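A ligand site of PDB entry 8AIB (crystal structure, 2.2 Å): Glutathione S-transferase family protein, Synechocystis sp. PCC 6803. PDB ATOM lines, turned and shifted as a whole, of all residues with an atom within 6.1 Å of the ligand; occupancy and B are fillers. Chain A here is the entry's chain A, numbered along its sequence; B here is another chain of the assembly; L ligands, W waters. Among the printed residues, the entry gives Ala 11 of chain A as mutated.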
ATOM      1  N   GLN A   9     -13.213  -0.347 -21.284  1.00  0.00           N
ATOM      2  CA  GLN A   9     -12.533  -1.440 -20.617  1.00  0.00           C
ATOM      3  C   GLN A   9     -13.503  -2.356 -19.837  1.00  0.00           C
ATOM      4  O   GLN A   9     -13.208  -2.789 -18.717  1.00  0.00           O
ATOM      5  CB  GLN A   9     -11.371  -0.901 -19.742  1.00  0.00           C
ATOM      6  CG  GLN A   9     -10.434   0.091 -20.461  1.00  0.00           C
ATOM      7  CD  GLN A   9      -9.865  -0.426 -21.777  1.00  0.00           C
ATOM      8  OE1 GLN A   9      -9.535  -1.618 -21.942  1.00  0.00           O
ATOM      9  NE2 GLN A   9      -9.721   0.474 -22.745  1.00  0.00           N
ATOM     10  N   SER A  10     -14.656  -2.632 -20.451  1.00  0.00           N
ATOM     11  CA  SER A  10     -15.632  -3.579 -19.907  1.00  0.00           C
ATOM     12  C   SER A  10     -15.941  -4.621 -21.009  1.00  0.00           C
ATOM     13  O   SER A  10     -15.489  -4.464 -22.151  1.00  0.00           O
ATOM     14  CB  SER A  10     -16.904  -2.861 -19.452  1.00  0.00           C
ATOM     15  OG  SER A  10     -17.740  -2.517 -20.555  1.00  0.00           O
ATOM     16  N   ALA A  11     -16.741  -5.653 -20.704  1.00  0.00           N
ATOM     17  CA  ALA A  11     -17.139  -6.637 -21.707  1.00  0.00           C
ATOM     18  C   ALA A  11     -18.206  -6.106 -22.675  1.00  0.00           C
ATOM     19  O   ALA A  11     -18.636  -6.867 -23.539  1.00  0.00           O
ATOM     20  CB  ALA A  11     -17.621  -7.918 -21.047  1.00  0.00           C
ATOM     21  N   LEU A  33     -18.789   4.329 -14.627  1.00  0.00           N
ATOM     22  CA  LEU A  33     -18.363   3.555 -13.476  1.00  0.00           C
ATOM     23  C   LEU A  33     -17.541   4.380 -12.499  1.00  0.00           C
ATOM     24  O   LEU A  33     -17.782   4.309 -11.301  1.00  0.00           O
ATOM     25  CB  LEU A  33     -17.588   2.290 -13.897  1.00  0.00           C
ATOM     26  CG  LEU A  33     -18.292   1.305 -14.856  1.00  0.00           C
ATOM     27  CD1 LEU A  33     -17.464   0.044 -15.034  1.00  0.00           C
ATOM     28  CD2 LEU A  33     -19.672   0.932 -14.371  1.00  0.00           C
ATOM     29  N   HIS A  38     -23.382   3.084 -12.155  1.00  0.00           N
ATOM     30  CA  HIS A  38     -23.824   1.701 -12.116  1.00  0.00           C
ATOM     31  C   HIS A  38     -24.428   1.330 -10.761  1.00  0.00           C
ATOM     32  O   HIS A  38     -25.185   0.378 -10.709  1.00  0.00           O
ATOM     33  CB  HIS A  38     -22.659   0.768 -12.487  1.00  0.00           C
ATOM     34  CG  HIS A  38     -21.494   0.886 -11.550  1.00  0.00           C
ATOM     35  ND1 HIS A  38     -20.881   2.108 -11.298  1.00  0.00           N
ATOM     36  CD2 HIS A  38     -20.850  -0.073 -10.844  1.00  0.00           C
ATOM     37  CE1 HIS A  38     -19.907   1.854 -10.441  1.00  0.00           C
ATOM     38  NE2 HIS A  38     -19.843   0.555 -10.150  1.00  0.00           N
ATOM     39  N   ARG A  39     -24.147   2.096  -9.678  1.00  0.00           N
ATOM     40  CA  ARG A  39     -24.724   1.821  -8.358  1.00  0.00           C
ATOM     41  C   ARG A  39     -25.937   2.709  -8.036  1.00  0.00           C
ATOM     42  O   ARG A  39     -26.320   2.823  -6.862  1.00  0.00           O
ATOM     43  CB  ARG A  39     -23.678   1.963  -7.256  1.00  0.00           C
ATOM     44  CG  ARG A  39     -22.367   1.212  -7.518  1.00  0.00           C
ATOM     45  CD  ARG A  39     -22.532  -0.284  -7.446  1.00  0.00           C
ATOM     46  NE  ARG A  39     -23.089  -0.719  -6.168  1.00  0.00           N
ATOM     47  CZ  ARG A  39     -23.661  -1.905  -5.954  1.00  0.00           C
ATOM     48  NH1 ARG A  39     -23.720  -2.804  -6.938  1.00  0.00           N
ATOM     49  NH2 ARG A  39     -24.169  -2.197  -4.765  1.00  0.00           N
ATOM     50  N   PHE A  49     -27.174  -6.236  -9.838  1.00  0.00           N
ATOM     51  CA  PHE A  49     -25.823  -6.415  -9.316  1.00  0.00           C
ATOM     52  C   PHE A  49     -24.872  -5.264  -9.728  1.00  0.00           C
ATOM     53  O   PHE A  49     -23.675  -5.344  -9.424  1.00  0.00           O
ATOM     54  CB  PHE A  49     -25.247  -7.793  -9.678  1.00  0.00           C
ATOM     55  CG  PHE A  49     -26.130  -8.879  -9.092  1.00  0.00           C
ATOM     56  CD1 PHE A  49     -26.039  -9.211  -7.750  1.00  0.00           C
ATOM     57  CD2 PHE A  49     -27.086  -9.504  -9.857  1.00  0.00           C
ATOM     58  CE1 PHE A  49     -26.886 -10.169  -7.189  1.00  0.00           C
ATOM     59  CE2 PHE A  49     -27.958 -10.447  -9.296  1.00  0.00           C
ATOM     60  CZ  PHE A  49     -27.865 -10.755  -7.972  1.00  0.00           C
ATOM     61  N   GLY A  50     -25.382  -4.257 -10.436  1.00  0.00           N
ATOM     62  CA  GLY A  50     -24.640  -3.086 -10.863  1.00  0.00           C
ATOM     63  C   GLY A  50     -23.433  -3.361 -11.721  1.00  0.00           C
ATOM     64  O   GLY A  50     -22.391  -2.725 -11.541  1.00  0.00           O
ATOM     65  N   LYS A  51     -23.549  -4.285 -12.661  1.00  0.00           N
ATOM     66  CA  LYS A  51     -22.449  -4.577 -13.570  1.00  0.00           C
ATOM     67  C   LYS A  51     -22.840  -4.337 -15.018  1.00  0.00           C
ATOM     68  O   LYS A  51     -23.984  -4.590 -15.403  1.00  0.00           O
ATOM     69  CB  LYS A  51     -22.013  -6.055 -13.435  1.00  0.00           C
ATOM     70  CG  LYS A  51     -21.747  -6.530 -12.012  1.00  0.00           C
ATOM     71  CD  LYS A  51     -20.348  -6.221 -11.605  1.00  0.00           C
ATOM     72  CE  LYS A  51     -20.079  -6.659 -10.182  1.00  0.00           C
ATOM     73  NZ  LYS A  51     -18.620  -6.618  -9.904  1.00  0.00           N
ATOM     74  N   VAL A  52     -21.874  -3.916 -15.836  1.00  0.00           N
ATOM     75  CA  VAL A  52     -22.030  -3.776 -17.289  1.00  0.00           C
ATOM     76  C   VAL A  52     -21.217  -4.958 -17.926  1.00  0.00           C
ATOM     77  O   VAL A  52     -20.245  -5.443 -17.338  1.00  0.00           O
ATOM     78  CB  VAL A  52     -21.552  -2.394 -17.835  1.00  0.00           C
ATOM     79  CG1 VAL A  52     -22.578  -1.295 -17.544  1.00  0.00           C
ATOM     80  CG2 VAL A  52     -20.170  -2.018 -17.293  1.00  0.00           C
ATOM     81  N   PRO A  53     -21.621  -5.472 -19.091  1.00  0.00           N
ATOM     82  CA  PRO A  53     -22.722  -4.980 -19.933  1.00  0.00           C
ATOM     83  C   PRO A  53     -24.091  -5.475 -19.540  1.00  0.00           C
ATOM     84  O   PRO A  53     -24.243  -6.336 -18.654  1.00  0.00           O
ATOM     85  CB  PRO A  53     -22.341  -5.511 -21.323  1.00  0.00           C
ATOM     86  CG  PRO A  53     -21.748  -6.867 -20.994  1.00  0.00           C
ATOM     87  CD  PRO A  53     -20.905  -6.574 -19.752  1.00  0.00           C
ATOM     88  N   TRP A  63     -28.666  -9.132 -18.549  1.00  0.00           N
ATOM     89  CA  TRP A  63     -27.298  -8.874 -18.147  1.00  0.00           C
ATOM     90  C   TRP A  63     -26.442 -10.195 -18.201  1.00  0.00           C
ATOM     91  O   TRP A  63     -26.985 -11.278 -18.511  1.00  0.00           O
ATOM     92  CB  TRP A  63     -27.207  -8.102 -16.797  1.00  0.00           C
ATOM     93  CG  TRP A  63     -28.148  -8.592 -15.736  1.00  0.00           C
ATOM     94  CD1 TRP A  63     -29.448  -8.207 -15.539  1.00  0.00           C
ATOM     95  CD2 TRP A  63     -27.868  -9.582 -14.753  1.00  0.00           C
ATOM     96  NE1 TRP A  63     -30.002  -8.932 -14.507  1.00  0.00           N
ATOM     97  CE2 TRP A  63     -29.050  -9.790 -14.012  1.00  0.00           C
ATOM     98  CE3 TRP A  63     -26.735 -10.359 -14.443  1.00  0.00           C
ATOM     99  CZ2 TRP A  63     -29.115 -10.698 -12.962  1.00  0.00           C
ATOM    100  CZ3 TRP A  63     -26.822 -11.271 -13.418  1.00  0.00           C
ATOM    101  CH2 TRP A  63     -27.992 -11.445 -12.698  1.00  0.00           C
ATOM    102  N   GLU A  64     -25.127 -10.093 -17.960  1.00  0.00           N
ATOM    103  CA  GLU A  64     -24.095 -11.127 -18.115  1.00  0.00           C
ATOM    104  C   GLU A  64     -23.758 -11.182 -19.580  1.00  0.00           C
ATOM    105  O   GLU A  64     -24.601 -11.577 -20.395  1.00  0.00           O
ATOM    106  CB  GLU A  64     -24.484 -12.529 -17.584  1.00  0.00           C
ATOM    107  CG  GLU A  64     -24.446 -12.667 -16.062  1.00  0.00           C
ATOM    108  CD  GLU A  64     -23.070 -12.472 -15.460  1.00  0.00           C
ATOM    109  OE1 GLU A  64     -22.070 -12.874 -16.096  1.00  0.00           O
ATOM    110  OE2 GLU A  64     -22.999 -11.923 -14.340  1.00  0.00           O
ATOM    111  N   SER A  65     -22.505 -10.792 -19.928  1.00  0.00           N
ATOM    112  CA  SER A  65     -21.999 -10.759 -21.291  1.00  0.00           C
ATOM    113  C   SER A  65     -22.204 -12.087 -22.010  1.00  0.00           C
ATOM    114  O   SER A  65     -22.583 -12.096 -23.190  1.00  0.00           O
ATOM    115  CB  SER A  65     -20.532 -10.345 -21.316  1.00  0.00           C
ATOM    116  OG  SER A  65     -19.698 -11.275 -20.632  1.00  0.00           O
ATOM    117  N   GLY A  66     -22.015 -13.200 -21.297  1.00  0.00           N
ATOM    118  CA  GLY A  66     -22.195 -14.514 -21.897  1.00  0.00           C
ATOM    119  C   GLY A  66     -23.636 -14.783 -22.306  1.00  0.00           C
ATOM    120  O   GLY A  66     -23.890 -15.248 -23.406  1.00  0.00           O
ATOM    121  N   ASN A  97     -16.150 -17.496 -19.788  1.00  0.00           N
ATOM    122  CA  ASN A  97     -16.457 -16.697 -18.616  1.00  0.00           C
ATOM    123  C   ASN A  97     -15.987 -17.239 -17.272  1.00  0.00           C
ATOM    124  O   ASN A  97     -15.973 -16.484 -16.285  1.00  0.00           O
ATOM    125  CB  ASN A  97     -17.955 -16.442 -18.562  1.00  0.00           C
ATOM    126  CG  ASN A  97     -18.331 -15.345 -19.533  1.00  0.00           C
ATOM    127  OD1 ASN A  97     -18.266 -14.145 -19.179  1.00  0.00           O
ATOM    128  ND2 ASN A  97     -18.678 -15.722 -20.776  1.00  0.00           N
ATOM    129  N   LEU B  94     -24.772 -18.039 -15.875  1.00  0.00           N
ATOM    130  CA  LEU B  94     -23.533 -17.302 -16.116  1.00  0.00           C
ATOM    131  C   LEU B  94     -23.101 -16.553 -14.856  1.00  0.00           C
ATOM    132  O   LEU B  94     -21.935 -16.564 -14.484  1.00  0.00           O
ATOM    133  CB  LEU B  94     -23.669 -16.313 -17.283  1.00  0.00           C
ATOM    134  CG  LEU B  94     -23.153 -16.827 -18.634  1.00  0.00           C
ATOM    135  CD1 LEU B  94     -21.662 -17.263 -18.545  1.00  0.00           C
ATOM    136  CD2 LEU B  94     -23.975 -17.992 -19.132  1.00  0.00           C
ATOM    137  N   PHE B  95     -24.070 -15.903 -14.190  1.00  0.00           N
ATOM    138  CA  PHE B  95     -23.875 -15.161 -12.967  1.00  0.00           C
ATOM    139  C   PHE B  95     -23.301 -16.084 -11.876  1.00  0.00           C
ATOM    140  O   PHE B  95     -22.356 -15.690 -11.199  1.00  0.00           O
ATOM    141  CB  PHE B  95     -25.235 -14.590 -12.516  1.00  0.00           C
ATOM    142  CG  PHE B  95     -25.204 -14.011 -11.130  1.00  0.00           C
ATOM    143  CD1 PHE B  95     -24.656 -12.760 -10.898  1.00  0.00           C
ATOM    144  CD2 PHE B  95     -25.764 -14.682 -10.061  1.00  0.00           C
ATOM    145  CE1 PHE B  95     -24.660 -12.204  -9.628  1.00  0.00           C
ATOM    146  CE2 PHE B  95     -25.755 -14.138  -8.789  1.00  0.00           C
ATOM    147  CZ  PHE B  95     -25.204 -12.905  -8.581  1.00  0.00           C
ATOM    148  N   SER B  98     -19.573 -17.043 -12.747  1.00  0.00           N
ATOM    149  CA  SER B  98     -18.548 -16.029 -12.916  1.00  0.00           C
ATOM    150  C   SER B  98     -18.675 -14.943 -11.827  1.00  0.00           C
ATOM    151  O   SER B  98     -17.995 -15.057 -10.822  1.00  0.00           O
ATOM    152  CB  SER B  98     -18.556 -15.444 -14.330  1.00  0.00           C
ATOM    153  OG  SER B  98     -19.831 -14.868 -14.589  1.00  0.00           O
ATOM    154  N   THR B  99     -19.596 -13.977 -11.979  1.00  0.00           N
ATOM    155  CA  THR B  99     -19.794 -12.869 -11.051  1.00  0.00           C
ATOM    156  C   THR B  99     -19.951 -13.302  -9.590  1.00  0.00           C
ATOM    157  O   THR B  99     -19.248 -12.779  -8.723  1.00  0.00           O
ATOM    158  CB  THR B  99     -20.989 -12.010 -11.523  1.00  0.00           C
ATOM    159  OG1 THR B  99     -20.807 -11.714 -12.913  1.00  0.00           O
ATOM    160  CG2 THR B  99     -21.162 -10.728 -10.695  1.00  0.00           C
ATOM    161  N   LYS B 112     -14.758  -6.472  -1.071  1.00  0.00           N
ATOM    162  CA  LYS B 112     -15.582  -5.536  -1.810  1.00  0.00           C
ATOM    163  C   LYS B 112     -16.864  -6.159  -2.431  1.00  0.00           C
ATOM    164  O   LYS B 112     -17.965  -5.636  -2.228  1.00  0.00           O
ATOM    165  CB  LYS B 112     -14.750  -4.824  -2.892  1.00  0.00           C
ATOM    166  CG  LYS B 112     -15.550  -3.742  -3.636  1.00  0.00           C
ATOM    167  CD  LYS B 112     -14.866  -3.275  -4.891  1.00  0.00           C
ATOM    168  CE  LYS B 112     -15.506  -2.034  -5.441  1.00  0.00           C
ATOM    169  NZ  LYS B 112     -14.757  -1.512  -6.616  1.00  0.00           N
ATOM    170  N   GLU B 113     -16.693  -7.263  -3.193  1.00  0.00           N
ATOM    171  CA  GLU B 113     -17.772  -7.926  -3.958  1.00  0.00           C
ATOM    172  C   GLU B 113     -18.840  -8.637  -3.135  1.00  0.00           C
ATOM    173  O   GLU B 113     -20.024  -8.419  -3.388  1.00  0.00           O
ATOM    174  CB  GLU B 113     -17.176  -8.941  -4.964  1.00  0.00           C
ATOM    175  CG  GLU B 113     -16.377  -8.337  -6.091  1.00  0.00           C
ATOM    176  CD  GLU B 113     -17.219  -7.365  -6.885  1.00  0.00           C
ATOM    177  OE1 GLU B 113     -18.215  -7.813  -7.491  1.00  0.00           O
ATOM    178  OE2 GLU B 113     -16.925  -6.145  -6.824  1.00  0.00           O
ATOM    179  N   ARG B 116     -21.791  -6.735  -1.483  1.00  0.00           N
ATOM    180  CA  ARG B 116     -22.631  -6.182  -2.560  1.00  0.00           C
ATOM    181  C   ARG B 116     -23.506  -7.264  -3.187  1.00  0.00           C
ATOM    182  O   ARG B 116     -24.704  -7.036  -3.413  1.00  0.00           O
ATOM    183  CB  ARG B 116     -21.780  -5.530  -3.652  1.00  0.00           C
ATOM    184  CG  ARG B 116     -21.147  -4.211  -3.238  1.00  0.00           C
ATOM    185  CD  ARG B 116     -20.214  -3.650  -4.291  1.00  0.00           C
ATOM    186  NE  ARG B 116     -19.947  -2.239  -4.032  1.00  0.00           N
ATOM    187  CZ  ARG B 116     -19.476  -1.383  -4.936  1.00  0.00           C
ATOM    188  NH1 ARG B 116     -19.189  -1.796  -6.166  1.00  0.00           N
ATOM    189  NH2 ARG B 116     -19.305  -0.103  -4.612  1.00  0.00           N
HETATM  190  N1  LIG L   1     -19.534 -11.873 -15.556  1.00  0.00           N
HETATM  191  C1  LIG L   1     -19.890 -10.459 -15.847  1.00  0.00           C
HETATM  192  C2  LIG L   1     -20.106 -10.302 -17.350  1.00  0.00           C
HETATM  193  O1  LIG L   1     -19.312 -10.918 -18.092  1.00  0.00           O
HETATM  194  O2  LIG L   1     -21.097  -9.630 -17.730  1.00  0.00           O
HETATM  195  C3  LIG L   1     -18.791  -9.500 -15.369  1.00  0.00           C
HETATM  196  C4  LIG L   1     -19.235  -8.050 -15.443  1.00  0.00           C
HETATM  197  C5  LIG L   1     -18.295  -7.104 -14.737  1.00  0.00           C
HETATM  198  O3  LIG L   1     -17.505  -7.487 -13.873  1.00  0.00           O
HETATM  199  N2  LIG L   1     -18.371  -5.824 -15.120  1.00  0.00           N
HETATM  200  C6  LIG L   1     -17.568  -4.772 -14.541  1.00  0.00           C
HETATM  201  C7  LIG L   1     -18.364  -3.782 -13.707  1.00  0.00           C
HETATM  202  O4  LIG L   1     -19.424  -3.329 -14.149  1.00  0.00           O
HETATM  203  C8  LIG L   1     -16.772  -4.055 -15.620  1.00  0.00           C
HETATM  204  S1  LIG L   1     -15.382  -5.014 -16.276  1.00  0.00           S
HETATM  205  N3  LIG L   1     -17.873  -3.467 -12.511  1.00  0.00           N
HETATM  206  C9  LIG L   1     -18.479  -2.459 -11.663  1.00  0.00           C
HETATM  207  C10 LIG L   1     -18.441  -2.850 -10.190  1.00  0.00           C
HETATM  208  O5  LIG L   1     -17.987  -3.974  -9.921  1.00  0.00           O
HETATM  209  O6  LIG L   1     -18.905  -2.046  -9.360  1.00  0.00           O
HETATM  210  O   HOH W   1     -21.078 -13.629 -18.562  1.00  0.00           O
HETATM  211  O   HOH W   2     -23.228  -8.186 -16.891  1.00  0.00           O
HETATM  212  O   HOH W   3     -17.425  -9.676 -11.626  1.00  0.00           O
HETATM  213  O   HOH W   4     -17.088 -11.956 -13.492  1.00  0.00           O
HETATM  214  O   HOH W   5     -19.070  -4.305  -7.333  1.00  0.00           O
HETATM  215  O   HOH W   6     -21.632  -3.091  -8.810  1.00  0.00           O
HETATM  216  O   HOH W   7     -17.243 -13.007 -16.894  1.00  0.00           O
HETATM  217  O   HOH W   8     -15.185  -4.731 -11.760  1.00  0.00           O
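N1 of the ligand sits at hydrogen-bond distance from OG1 of Thr 99 of chain B, at 2.9 Å.
NE2 of His 38 lies within hydrogen-bond range of O6 of the ligand.
The backbone NH (N) of Val 52 lies within hydrogen-bond range of an oxygen (O4) of the ligand.
N2 of the ligand sits at hydrogen-bond distance from O of Val 52, 2.9 Å away.
A nitrogen (N1) of the ligand lies within hydrogen-bond range of the side-chain hydroxyl of Ser 98 of chain B, 3.2 Å away.
N of Ser 65 lies within hydrogen-bond range of O2 of the ligand, at 2.9 Å.
An oxygen (O1) of the ligand lies within hydrogen-bond range of the side-chain hydroxyl (OG) of Ser 65 (2.6 Å).
NH1 of Arg 116 of chain B lies within salt-bridge range of O6 of the ligand, 3.2 Å away.
The side-chain carboxylate (OE1) of Glu 64 is in salt-bridge range of a nitrogen (N1) of the ligand, at 2.8 Å.
The side-chain amino group of Lys 51 is in salt-bridge range of an oxygen (O5) of the ligand (2.7 Å).
OE1 of Glu 113 of chain B is in salt-bridge range of NZ of Lys 51 (2.7 Å).
The side-chain hydroxyl (OG) of Ser 98 of chain B is in hydrogen-bond range of the side-chain carboxylate (OE1) of Glu 64 (3.4 Å).
The side-chain hydroxyl (OG) of Ser 98 of chain B lies within hydrogen-bond range of the backbone carbonyl oxygen (O) of Leu 94 of chain B, 2.7 Å away.
OE2 of Glu 64 lies within hydrogen-bond range of OG1 of Thr 99 of chain B (2.6 Å).
Merely in contact with the ligand: Gln 9 (3.95 Å), Ser 10 (3.9 Å), Gly 50 (3.9 Å), Pro 53 (3.7 Å), Asn 97 (3.6 Å) and Glu 113 of chain B (3.9 Å).
Hydrophobic or aromatic side chains within 4 Å of the ligand: His 38, Val 52 and Pro 53.
14 residues have an atom within 4 Å of the ligand: Gln 9, Ser 10, His 38, Gly 50, Lys 51, Val 52, Pro 53, Glu 64, Ser 65, Asn 97, Ser 98 of chain B, Thr 99 of chain B, Glu 113 of chain B and Arg 116 of chain B.
The nearest printed residue that does not touch the ligand is Leu 33 (4.0002 Å).
Water W2 lies within hydrogen-bond range of an oxygen (O2) of the ligand (2.7 Å), the backbone carbonyl oxygen (O) of Pro 53 (2.7 Å) and the backbone NH (N) of Glu 64 (2.9 Å).
Water W5 lies within hydrogen-bond range of the guanidinium group (NH1) of Arg 116 of chain B, an oxygen (O5) of the ligand, the side-chain carboxylate (OE2) of Glu 113 of chain B and the side-chain amino group (NZ) of Lys 51.
Water W7 lies within hydrogen-bond range of the side-chain amide oxygen (OD1) of Asn 97 (2.8 Å) and a nitrogen (N1) of the ligand (2.9 Å).
Water W6 lies within hydrogen-bond range of NH1 of Arg 39, O of Gly 50, O6 of the ligand and O of Phe 49.
Water W1 lies within hydrogen-bond range of the side-chain carboxylate of Glu 64 (2.8 Å), the backbone NH of Gly 66 (2.9 Å), the side-chain amide oxygen of Asn 97 (2.9 Å), an oxygen (O1) of the ligand (3.3 Å) and the side-chain hydroxyl of Ser 65 (3.4 Å).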
